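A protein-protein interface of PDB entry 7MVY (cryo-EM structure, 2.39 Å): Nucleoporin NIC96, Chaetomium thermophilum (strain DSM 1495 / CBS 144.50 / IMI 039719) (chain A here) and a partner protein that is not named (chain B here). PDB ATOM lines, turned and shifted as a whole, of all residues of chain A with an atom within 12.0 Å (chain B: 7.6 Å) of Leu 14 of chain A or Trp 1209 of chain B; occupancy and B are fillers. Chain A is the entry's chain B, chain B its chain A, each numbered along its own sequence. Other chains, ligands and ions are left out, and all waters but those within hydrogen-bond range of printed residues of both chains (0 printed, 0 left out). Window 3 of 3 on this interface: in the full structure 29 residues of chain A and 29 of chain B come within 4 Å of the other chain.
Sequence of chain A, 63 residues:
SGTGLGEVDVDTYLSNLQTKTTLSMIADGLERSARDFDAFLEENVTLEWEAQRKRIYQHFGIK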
ATOM      1  N   ASP A   9     -12.795  22.250 -21.006  1.00  0.00           N
ATOM      2  CA  ASP A   9     -11.638  21.811 -20.235  1.00  0.00           C
ATOM      3  C   ASP A   9     -11.536  22.602 -18.936  1.00  0.00           C
ATOM      4  O   ASP A   9     -11.383  22.025 -17.857  1.00  0.00           O
ATOM      5  CB  ASP A   9     -10.355  21.971 -21.057  1.00  0.00           C
ATOM      6  CG  ASP A   9      -9.164  21.271 -20.426  1.00  0.00           C
ATOM      7  OD1 ASP A   9      -9.133  21.135 -19.185  1.00  0.00           O
ATOM      8  OD2 ASP A   9      -8.258  20.852 -21.176  1.00  0.00           O
ATOM      9  N   VAL A  10     -11.623  23.929 -19.045  1.00  0.00           N
ATOM     10  CA  VAL A  10     -11.536  24.778 -17.860  1.00  0.00           C
ATOM     11  C   VAL A  10     -12.714  24.512 -16.931  1.00  0.00           C
ATOM     12  O   VAL A  10     -12.576  24.553 -15.702  1.00  0.00           O
ATOM     13  CB  VAL A  10     -11.462  26.261 -18.269  1.00  0.00           C
ATOM     14  CG1 VAL A  10     -11.377  27.151 -17.036  1.00  0.00           C
ATOM     15  CG2 VAL A  10     -10.273  26.500 -19.188  1.00  0.00           C
ATOM     16  N   ASP A  11     -13.888  24.234 -17.500  1.00  0.00           N
ATOM     17  CA  ASP A  11     -15.055  23.932 -16.677  1.00  0.00           C
ATOM     18  C   ASP A  11     -14.800  22.713 -15.800  1.00  0.00           C
ATOM     19  O   ASP A  11     -15.008  22.754 -14.582  1.00  0.00           O
ATOM     20  CB  ASP A  11     -16.278  23.709 -17.568  1.00  0.00           C
ATOM     21  CG  ASP A  11     -16.614  24.925 -18.409  1.00  0.00           C
ATOM     22  OD1 ASP A  11     -16.336  26.056 -17.959  1.00  0.00           O
ATOM     23  OD2 ASP A  11     -17.157  24.749 -19.520  1.00  0.00           O
ATOM     24  N   THR A  12     -14.343  21.614 -16.405  1.00  0.00           N
ATOM     25  CA  THR A  12     -14.061  20.409 -15.630  1.00  0.00           C
ATOM     26  C   THR A  12     -12.916  20.641 -14.651  1.00  0.00           C
ATOM     27  O   THR A  12     -12.944  20.140 -13.521  1.00  0.00           O
ATOM     28  CB  THR A  12     -13.733  19.246 -16.567  1.00  0.00           C
ATOM     29  OG1 THR A  12     -12.591  19.578 -17.367  1.00  0.00           O
ATOM     30  CG2 THR A  12     -14.916  18.938 -17.474  1.00  0.00           C
ATOM     31  N   TYR A  13     -11.896  21.395 -15.070  1.00  0.00           N
ATOM     32  CA  TYR A  13     -10.776  21.680 -14.180  1.00  0.00           C
ATOM     33  C   TYR A  13     -11.242  22.407 -12.926  1.00  0.00           C
ATOM     34  O   TYR A  13     -10.802  22.091 -11.814  1.00  0.00           O
ATOM     35  CB  TYR A  13      -9.719  22.504 -14.916  1.00  0.00           C
ATOM     36  CG  TYR A  13      -8.554  22.923 -14.047  1.00  0.00           C
ATOM     37  CD1 TYR A  13      -7.478  22.071 -13.837  1.00  0.00           C
ATOM     38  CD2 TYR A  13      -8.530  24.170 -13.438  1.00  0.00           C
ATOM     39  CE1 TYR A  13      -6.411  22.450 -13.045  1.00  0.00           C
ATOM     40  CE2 TYR A  13      -7.468  24.558 -12.643  1.00  0.00           C
ATOM     41  CZ  TYR A  13      -6.412  23.694 -12.451  1.00  0.00           C
ATOM     42  OH  TYR A  13      -5.352  24.074 -11.660  1.00  0.00           O
ATOM     43  N   LEU A  14     -12.134  23.388 -13.084  1.00  0.00           N
ATOM     44  CA  LEU A  14     -12.640  24.117 -11.926  1.00  0.00           C
ATOM     45  C   LEU A  14     -13.633  23.281 -11.127  1.00  0.00           C
ATOM     46  O   LEU A  14     -13.757  23.465  -9.911  1.00  0.00           O
ATOM     47  CB  LEU A  14     -13.292  25.425 -12.373  1.00  0.00           C
ATOM     48  CG  LEU A  14     -12.372  26.437 -13.063  1.00  0.00           C
ATOM     49  CD1 LEU A  14     -13.169  27.636 -13.550  1.00  0.00           C
ATOM     50  CD2 LEU A  14     -11.254  26.880 -12.130  1.00  0.00           C
ATOM     51  N   SER A  15     -14.344  22.364 -11.786  1.00  0.00           N
ATOM     52  CA  SER A  15     -15.303  21.526 -11.072  1.00  0.00           C
ATOM     53  C   SER A  15     -14.595  20.514 -10.180  1.00  0.00           C
ATOM     54  O   SER A  15     -15.006  20.296  -9.035  1.00  0.00           O
ATOM     55  CB  SER A  15     -16.218  20.815 -12.068  1.00  0.00           C
ATOM     56  OG  SER A  15     -16.938  21.749 -12.854  1.00  0.00           O
ATOM     57  N   ASN A  16     -13.532  19.887 -10.684  1.00  0.00           N
ATOM     58  CA  ASN A  16     -12.793  18.881  -9.935  1.00  0.00           C
ATOM     59  C   ASN A  16     -11.617  19.471  -9.162  1.00  0.00           C
ATOM     60  O   ASN A  16     -10.656  18.750  -8.869  1.00  0.00           O
ATOM     61  CB  ASN A  16     -12.297  17.782 -10.879  1.00  0.00           C
ATOM     62  CG  ASN A  16     -11.154  18.242 -11.762  1.00  0.00           C
ATOM     63  OD1 ASN A  16     -10.981  19.437 -12.002  1.00  0.00           O
ATOM     64  ND2 ASN A  16     -10.366  17.293 -12.252  1.00  0.00           N
ATOM     65  N   LEU A  17     -11.673  20.755  -8.827  1.00  0.00           N
ATOM     66  CA  LEU A  17     -10.600  21.410  -8.094  1.00  0.00           C
ATOM     67  C   LEU A  17     -10.872  21.361  -6.596  1.00  0.00           C
ATOM     68  O   LEU A  17     -12.021  21.410  -6.150  1.00  0.00           O
ATOM     69  CB  LEU A  17     -10.447  22.863  -8.549  1.00  0.00           C
ATOM     70  CG  LEU A  17      -9.321  23.666  -7.892  1.00  0.00           C
ATOM     71  CD1 LEU A  17      -7.965  23.045  -8.188  1.00  0.00           C
ATOM     72  CD2 LEU A  17      -9.361  25.114  -8.357  1.00  0.00           C
ATOM     73  N   GLN A  18      -9.794  21.263  -5.821  1.00  0.00           N
ATOM     74  CA  GLN A  18      -9.864  21.212  -4.368  1.00  0.00           C
ATOM     75  C   GLN A  18      -9.114  22.399  -3.781  1.00  0.00           C
ATOM     76  O   GLN A  18      -8.017  22.739  -4.235  1.00  0.00           O
ATOM     77  CB  GLN A  18      -9.276  19.902  -3.833  1.00  0.00           C
ATOM     78  CG  GLN A  18      -7.829  19.658  -4.237  1.00  0.00           C
ATOM     79  CD  GLN A  18      -7.294  18.337  -3.718  1.00  0.00           C
ATOM     80  OE1 GLN A  18      -8.001  17.591  -3.042  1.00  0.00           O
ATOM     81  NE2 GLN A  18      -6.038  18.043  -4.033  1.00  0.00           N
ATOM     82  N   THR A  19      -9.711  23.025  -2.771  1.00  0.00           N
ATOM     83  CA  THR A  19      -9.109  24.183  -2.109  1.00  0.00           C
ATOM     84  C   THR A  19      -7.996  23.692  -1.191  1.00  0.00           C
ATOM     85  O   THR A  19      -8.243  23.263  -0.061  1.00  0.00           O
ATOM     86  CB  THR A  19     -10.162  24.979  -1.342  1.00  0.00           C
ATOM     87  OG1 THR A  19      -9.544  26.111  -0.716  1.00  0.00           O
ATOM     88  CG2 THR A  19     -10.846  24.123  -0.275  1.00  0.00           C
ATOM     89  N   LYS A  20      -6.761  23.747  -1.679  1.00  0.00           N
ATOM     90  CA  LYS A  20      -5.605  23.312  -0.905  1.00  0.00           C
ATOM     91  C   LYS A  20      -4.347  23.746  -1.642  1.00  0.00           C
ATOM     92  O   LYS A  20      -4.356  23.941  -2.861  1.00  0.00           O
ATOM     93  CB  LYS A  20      -5.613  21.796  -0.687  1.00  0.00           C
ATOM     94  CG  LYS A  20      -4.488  21.290   0.202  1.00  0.00           C
ATOM     95  CD  LYS A  20      -4.665  19.818   0.538  1.00  0.00           C
ATOM     96  CE  LYS A  20      -3.532  19.307   1.414  1.00  0.00           C
ATOM     97  NZ  LYS A  20      -3.713  17.877   1.787  1.00  0.00           N
ATOM     98  N   THR A  21      -3.264  23.898  -0.882  1.00  0.00           N
ATOM     99  CA  THR A  21      -2.002  24.334  -1.464  1.00  0.00           C
ATOM    100  C   THR A  21      -1.532  23.344  -2.523  1.00  0.00           C
ATOM    101  O   THR A  21      -1.741  22.135  -2.406  1.00  0.00           O
ATOM    102  CB  THR A  21      -0.938  24.484  -0.373  1.00  0.00           C
ATOM    103  OG1 THR A  21       0.256  25.037  -0.939  1.00  0.00           O
ATOM    104  CG2 THR A  21      -0.619  23.135   0.260  1.00  0.00           C
ATOM    105  N   THR A  22      -0.890  23.871  -3.568  1.00  0.00           N
ATOM    106  CA  THR A  22      -0.440  23.026  -4.669  1.00  0.00           C
ATOM    107  C   THR A  22       0.827  22.258  -4.309  1.00  0.00           C
ATOM    108  O   THR A  22       0.985  21.100  -4.712  1.00  0.00           O
ATOM    109  CB  THR A  22      -0.204  23.876  -5.919  1.00  0.00           C
ATOM    110  OG1 THR A  22      -1.422  24.534  -6.292  1.00  0.00           O
ATOM    111  CG2 THR A  22       0.276  23.008  -7.076  1.00  0.00           C
ATOM    112  N   LEU A  23       1.737  22.882  -3.558  1.00  0.00           N
ATOM    113  CA  LEU A  23       2.991  22.224  -3.207  1.00  0.00           C
ATOM    114  C   LEU A  23       2.784  20.971  -2.365  1.00  0.00           C
ATOM    115  O   LEU A  23       3.730  20.193  -2.204  1.00  0.00           O
ATOM    116  CB  LEU A  23       3.912  23.204  -2.471  1.00  0.00           C
ATOM    117  CG  LEU A  23       3.354  23.964  -1.262  1.00  0.00           C
ATOM    118  CD1 LEU A  23       3.129  23.046  -0.068  1.00  0.00           C
ATOM    119  CD2 LEU A  23       4.285  25.109  -0.889  1.00  0.00           C
ATOM    120  N   MET A  25       0.157  18.682  -3.051  1.00  0.00           N
ATOM    121  CA  MET A  25      -0.260  17.621  -3.960  1.00  0.00           C
ATOM    122  C   MET A  25       0.941  17.016  -4.677  1.00  0.00           C
ATOM    123  O   MET A  25       1.069  15.789  -4.770  1.00  0.00           O
ATOM    124  CB  MET A  25      -1.271  18.166  -4.971  1.00  0.00           C
ATOM    125  CG  MET A  25      -2.492  18.830  -4.348  1.00  0.00           C
ATOM    126  SD  MET A  25      -3.461  17.730  -3.295  1.00  0.00           S
ATOM    127  CE  MET A  25      -2.669  17.970  -1.706  1.00  0.00           C
ATOM    128  N   GLY B1145      -9.571  37.465  -3.654  1.00  0.00           N
ATOM    129  CA  GLY B1145     -10.254  37.486  -4.937  1.00  0.00           C
ATOM    130  C   GLY B1145     -10.382  38.888  -5.501  1.00  0.00           C
ATOM    131  O   GLY B1145     -10.140  39.113  -6.689  1.00  0.00           O
ATOM    132  N   LEU B1148      -6.904  39.863  -6.807  1.00  0.00           N
ATOM    133  CA  LEU B1148      -6.405  39.158  -7.982  1.00  0.00           C
ATOM    134  C   LEU B1148      -7.265  39.441  -9.208  1.00  0.00           C
ATOM    135  O   LEU B1148      -6.760  39.911 -10.234  1.00  0.00           O
ATOM    136  CB  LEU B1148      -6.344  37.653  -7.707  1.00  0.00           C
ATOM    137  CG  LEU B1148      -5.030  37.131  -7.116  1.00  0.00           C
ATOM    138  CD1 LEU B1148      -4.722  37.783  -5.776  1.00  0.00           C
ATOM    139  CD2 LEU B1148      -5.078  35.617  -6.976  1.00  0.00           C
ATOM    140  N   THR B1149      -8.568  39.161  -9.123  1.00  0.00           N
ATOM    141  CA  THR B1149      -9.444  39.388 -10.267  1.00  0.00           C
ATOM    142  C   THR B1149      -9.560  40.871 -10.599  1.00  0.00           C
ATOM    143  O   THR B1149      -9.713  41.231 -11.771  1.00  0.00           O
ATOM    144  CB  THR B1149     -10.830  38.801  -9.994  1.00  0.00           C
ATOM    145  OG1 THR B1149     -10.710  37.404  -9.698  1.00  0.00           O
ATOM    146  CG2 THR B1149     -11.741  38.984 -11.200  1.00  0.00           C
ATOM    147  N   VAL B1169      -9.133  36.392 -14.231  1.00  0.00           N
ATOM    148  CA  VAL B1169      -8.796  37.112 -15.452  1.00  0.00           C
ATOM    149  C   VAL B1169      -7.828  38.245 -15.131  1.00  0.00           C
ATOM    150  O   VAL B1169      -6.618  38.108 -15.311  1.00  0.00           O
ATOM    151  CB  VAL B1169     -10.061  37.647 -16.149  1.00  0.00           C
ATOM    152  CG1 VAL B1169      -9.691  38.423 -17.405  1.00  0.00           C
ATOM    153  CG2 VAL B1169     -11.008  36.503 -16.481  1.00  0.00           C
ATOM    154  N   ALA B1203       0.513  33.618  -4.806  1.00  0.00           N
ATOM    155  CA  ALA B1203      -0.753  33.658  -5.530  1.00  0.00           C
ATOM    156  C   ALA B1203      -1.003  32.374  -6.310  1.00  0.00           C
ATOM    157  O   ALA B1203      -2.159  32.033  -6.580  1.00  0.00           O
ATOM    158  CB  ALA B1203      -0.778  34.858  -6.478  1.00  0.00           C
ATOM    159  N   GLN B1204       0.059  31.655  -6.676  1.00  0.00           N
ATOM    160  CA  GLN B1204      -0.101  30.420  -7.435  1.00  0.00           C
ATOM    161  C   GLN B1204      -0.468  29.249  -6.531  1.00  0.00           C
ATOM    162  O   GLN B1204      -1.418  28.511  -6.815  1.00  0.00           O
ATOM    163  CB  GLN B1204       1.186  30.112  -8.205  1.00  0.00           C
ATOM    164  CG  GLN B1204       1.394  30.976  -9.437  1.00  0.00           C
ATOM    165  CD  GLN B1204       2.692  30.663 -10.155  1.00  0.00           C
ATOM    166  OE1 GLN B1204       3.455  29.795  -9.732  1.00  0.00           O
ATOM    167  NE2 GLN B1204       2.950  31.372 -11.248  1.00  0.00           N
ATOM    168  N   ASN B1205       0.273  29.062  -5.435  1.00  0.00           N
ATOM    169  CA  ASN B1205       0.052  27.889  -4.595  1.00  0.00           C
ATOM    170  C   ASN B1205      -1.334  27.897  -3.964  1.00  0.00           C
ATOM    171  O   ASN B1205      -1.923  26.831  -3.752  1.00  0.00           O
ATOM    172  CB  ASN B1205       1.129  27.807  -3.513  1.00  0.00           C
ATOM    173  CG  ASN B1205       1.115  29.002  -2.585  1.00  0.00           C
ATOM    174  OD1 ASN B1205       0.656  30.082  -2.954  1.00  0.00           O
ATOM    175  ND2 ASN B1205       1.623  28.816  -1.372  1.00  0.00           N
ATOM    176  N   TYR B1206      -1.873  29.078  -3.661  1.00  0.00           N
ATOM    177  CA  TYR B1206      -3.197  29.189  -3.060  1.00  0.00           C
ATOM    178  C   TYR B1206      -4.296  29.484  -4.070  1.00  0.00           C
ATOM    179  O   TYR B1206      -5.436  29.052  -3.868  1.00  0.00           O
ATOM    180  CB  TYR B1206      -3.200  30.283  -1.985  1.00  0.00           C
ATOM    181  CG  TYR B1206      -2.559  29.856  -0.684  1.00  0.00           C
ATOM    182  CD1 TYR B1206      -1.199  30.025  -0.467  1.00  0.00           C
ATOM    183  CD2 TYR B1206      -3.317  29.280   0.328  1.00  0.00           C
ATOM    184  CE1 TYR B1206      -0.609  29.635   0.722  1.00  0.00           C
ATOM    185  CE2 TYR B1206      -2.737  28.888   1.520  1.00  0.00           C
ATOM    186  CZ  TYR B1206      -1.383  29.067   1.711  1.00  0.00           C
ATOM    187  OH  TYR B1206      -0.802  28.677   2.895  1.00  0.00           O
ATOM    188  N   TRP B1207      -3.989  30.205  -5.147  1.00  0.00           N
ATOM    189  CA  TRP B1207      -4.956  30.528  -6.195  1.00  0.00           C
ATOM    190  C   TRP B1207      -4.354  30.165  -7.546  1.00  0.00           C
ATOM    191  O   TRP B1207      -4.068  31.038  -8.374  1.00  0.00           O
ATOM    192  CB  TRP B1207      -5.345  32.006  -6.146  1.00  0.00           C
ATOM    193  CG  TRP B1207      -5.992  32.410  -4.856  1.00  0.00           C
ATOM    194  CD1 TRP B1207      -5.364  32.853  -3.729  1.00  0.00           C
ATOM    195  CD2 TRP B1207      -7.394  32.408  -4.561  1.00  0.00           C
ATOM    196  NE1 TRP B1207      -6.289  33.127  -2.749  1.00  0.00           N
ATOM    197  CE2 TRP B1207      -7.542  32.861  -3.235  1.00  0.00           C
ATOM    198  CE3 TRP B1207      -8.538  32.066  -5.288  1.00  0.00           C
ATOM    199  CZ2 TRP B1207      -8.788  32.982  -2.622  1.00  0.00           C
ATOM    200  CZ3 TRP B1207      -9.774  32.187  -4.678  1.00  0.00           C
ATOM    201  CH2 TRP B1207      -9.889  32.642  -3.358  1.00  0.00           C
ATOM    202  N   PRO B1208      -4.148  28.870  -7.803  1.00  0.00           N
ATOM    203  CA  PRO B1208      -3.522  28.481  -9.077  1.00  0.00           C
ATOM    204  C   PRO B1208      -4.440  28.642 -10.275  1.00  0.00           C
ATOM    205  O   PRO B1208      -3.992  29.101 -11.333  1.00  0.00           O
ATOM    206  CB  PRO B1208      -3.145  27.013  -8.841  1.00  0.00           C
ATOM    207  CG  PRO B1208      -4.136  26.532  -7.836  1.00  0.00           C
ATOM    208  CD  PRO B1208      -4.432  27.707  -6.944  1.00  0.00           C
ATOM    209  N   TRP B1209      -5.719  28.282 -10.137  1.00  0.00           N
ATOM    210  CA  TRP B1209      -6.629  28.283 -11.278  1.00  0.00           C
ATOM    211  C   TRP B1209      -6.675  29.627 -11.993  1.00  0.00           C
ATOM    212  O   TRP B1209      -7.020  29.675 -13.179  1.00  0.00           O
ATOM    213  CB  TRP B1209      -8.037  27.895 -10.821  1.00  0.00           C
ATOM    214  CG  TRP B1209      -8.644  28.861  -9.849  1.00  0.00           C
ATOM    215  CD1 TRP B1209      -8.437  28.906  -8.501  1.00  0.00           C
ATOM    216  CD2 TRP B1209      -9.561  29.920 -10.151  1.00  0.00           C
ATOM    217  NE1 TRP B1209      -9.167  29.930  -7.945  1.00  0.00           N
ATOM    218  CE2 TRP B1209      -9.865  30.567  -8.936  1.00  0.00           C
ATOM    219  CE3 TRP B1209     -10.152  30.385 -11.329  1.00  0.00           C
ATOM    220  CZ2 TRP B1209     -10.735  31.653  -8.867  1.00  0.00           C
ATOM    221  CZ3 TRP B1209     -11.016  31.464 -11.258  1.00  0.00           C
ATOM    222  CH2 TRP B1209     -11.299  32.085 -10.035  1.00  0.00           C
ATOM    223  N   THR B1210      -6.335  30.717 -11.306  1.00  0.00           N
ATOM    224  CA  THR B1210      -6.331  32.048 -11.902  1.00  0.00           C
ATOM    225  C   THR B1210      -4.950  32.457 -12.401  1.00  0.00           C
ATOM    226  O   THR B1210      -4.808  32.887 -13.550  1.00  0.00           O
ATOM    227  CB  THR B1210      -6.839  33.079 -10.885  1.00  0.00           C
ATOM    228  OG1 THR B1210      -8.155  32.718 -10.449  1.00  0.00           O
ATOM    229  CG2 THR B1210      -6.876  34.471 -11.502  1.00  0.00           C
ATOM    230  N   ILE B1211      -3.925  32.328 -11.557  1.00  0.00           N
ATOM    231  CA  ILE B1211      -2.590  32.778 -11.936  1.00  0.00           C
ATOM    232  C   ILE B1211      -2.055  31.944 -13.093  1.00  0.00           C
ATOM    233  O   ILE B1211      -1.553  32.484 -14.087  1.00  0.00           O
ATOM    234  CB  ILE B1211      -1.642  32.730 -10.724  1.00  0.00           C
ATOM    235  CG1 ILE B1211      -2.211  33.546  -9.558  1.00  0.00           C
ATOM    236  CG2 ILE B1211      -0.264  33.244 -11.110  1.00  0.00           C
ATOM    237  CD1 ILE B1211      -2.449  35.011  -9.876  1.00  0.00           C
ATOM    238  N   PHE B1212      -2.144  30.616 -12.982  1.00  0.00           N
ATOM    239  CA  PHE B1212      -1.647  29.759 -14.053  1.00  0.00           C
ATOM    240  C   PHE B1212      -2.441  29.966 -15.335  1.00  0.00           C
ATOM    241  O   PHE B1212      -1.877  29.929 -16.435  1.00  0.00           O
ATOM    242  CB  PHE B1212      -1.696  28.293 -13.622  1.00  0.00           C
ATOM    243  CG  PHE B1212      -0.677  27.935 -12.581  1.00  0.00           C
ATOM    244  CD1 PHE B1212       0.630  27.651 -12.942  1.00  0.00           C
ATOM    245  CD2 PHE B1212      -1.025  27.880 -11.244  1.00  0.00           C
ATOM    246  CE1 PHE B1212       1.571  27.322 -11.986  1.00  0.00           C
ATOM    247  CE2 PHE B1212      -0.089  27.551 -10.284  1.00  0.00           C
ATOM    248  CZ  PHE B1212       1.210  27.271 -10.656  1.00  0.00           C
ATOM    249  N   ALA B1213      -3.750  30.191 -15.218  1.00  0.00           N
ATOM    250  CA  ALA B1213      -4.561  30.450 -16.403  1.00  0.00           C
ATOM    251  C   ALA B1213      -4.110  31.728 -17.100  1.00  0.00           C
ATOM    252  O   ALA B1213      -3.901  31.747 -18.319  1.00  0.00           O
ATOM    253  CB  ALA B1213      -6.037  30.537 -16.017  1.00  0.00           C
ATOM    254  N   VAL B1214      -3.949  32.811 -16.335  1.00  0.00           N
ATOM    255  CA  VAL B1214      -3.525  34.078 -16.925  1.00  0.00           C
ATOM    256  C   VAL B1214      -2.123  33.960 -17.506  1.00  0.00           C
ATOM    257  O   VAL B1214      -1.802  34.612 -18.506  1.00  0.00           O
ATOM    258  CB  VAL B1214      -3.607  35.206 -15.877  1.00  0.00           C
ATOM    259  CG1 VAL B1214      -2.997  36.489 -16.427  1.00  0.00           C
ATOM    260  CG2 VAL B1214      -5.052  35.439 -15.460  1.00  0.00           C
ATOM    261  N   HIS B1266       0.571  21.299 -12.942  1.00  0.00           N
ATOM    262  CA  HIS B1266      -0.789  21.611 -13.373  1.00  0.00           C
ATOM    263  C   HIS B1266      -1.040  21.124 -14.795  1.00  0.00           C
ATOM    264  O   HIS B1266      -2.111  20.584 -15.096  1.00  0.00           O
ATOM    265  CB  HIS B1266      -1.045  23.115 -13.269  1.00  0.00           C
ATOM    266  CG  HIS B1266      -1.240  23.597 -11.866  1.00  0.00           C
ATOM    267  ND1 HIS B1266      -2.374  23.318 -11.135  1.00  0.00           N
ATOM    268  CD2 HIS B1266      -0.449  24.345 -11.061  1.00  0.00           C
ATOM    269  CE1 HIS B1266      -2.272  23.870  -9.939  1.00  0.00           C
ATOM    270  NE2 HIS B1266      -1.113  24.500  -9.868  1.00  0.00           N
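The backbone carbonyl oxygen (O) of Asn 1205 of chain B sits at hydrogen-bond distance from the backbone NH (N) of Thr 22 of chain A (3.1 Å).
ND1 of His 1266 of chain B is in hydrogen-bond range of OH of Tyr 13 of chain A (3.1 Å).
The side-chain amide oxygen of Asn 16 of chain A lies close to the backbone carbonyl oxygen of Tyr 13 of chain A (2.7 Å).
Tyr 13 of chain A touches Trp 1209 of chain B.
Trp 1209 of chain B touches Leu 14 of chain A (CB to CD2, 3.6 Å).
Trp 1209 of chain B touches Leu 17 of chain A (CD1 to CD2, 3.9 Å).
Lys 20 of chain A touches Asn 1205 of chain B (O to O, 3.9 Å).
Thr 21 of chain A touches Asn 1205 of chain B (CA to O, 3.4 Å).
Thr 22 of chain A touches Pro 1208 of chain B (OG1 to CG, 3.7 Å).
CG2 of Thr 22 of chain A touches NE2 of His 1266 of chain B, at 3.5 Å.
Of chain B, only Trp 1209 comes within 4 Å of Leu 14 of chain A.
Of the printed residues of chain B, Leu 17 of chain A touches Trp 1209.
Of the printed residues of chain B, Lys 20 of chain A touches Asn 1205.
Met 25 of chain A touches none of the printed residues of chain B.
Leu 1148 of chain B touches none of the printed residues of chain A.
Printed residues of chain A within 4 Å of Asn 1205 of chain B: Lys 20 (3.9 Å), Thr 21 (3.4 Å) and Thr 22 (3.1 Å).
No residue of chain A comes within 4 Å of Trp 1207 of chain B.
Pro 1208 of chain B touches just one residue of chain A: Thr 22.
Trp 1209 of chain B touches just these residues of chain A: Tyr 13, Leu 14 and Leu 17.
No residue of chain A comes within 4 Å of Thr 1210 of chain B.
No residue of chain A comes within 4 Å of Ile 1211 of chain B.
No residue of chain A comes within 4 Å of Phe 1212 of chain B.
No residue of chain A comes within 4 Å of Ala 1213 of chain B.
The nearest printed residue of chain B that does not touch Tyr 13 of chain A is Pro 1208 of chain B (4.6 Å).
Of the 17 printed residues of chain B, 4 touch a printed residue of chain A.
Hydrophobic or aromatic side chains of chain B that line the printed part of chain A: Pro 1208, Trp 1209 and His 1266.
Of the 16 printed residues of chain A, 6 touch a printed residue of chain B.
Along chain A the printed residues that touch a printed residue of chain B span positions 13 to 22.
Among the printed residues, 9 pairs touch across the chains.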
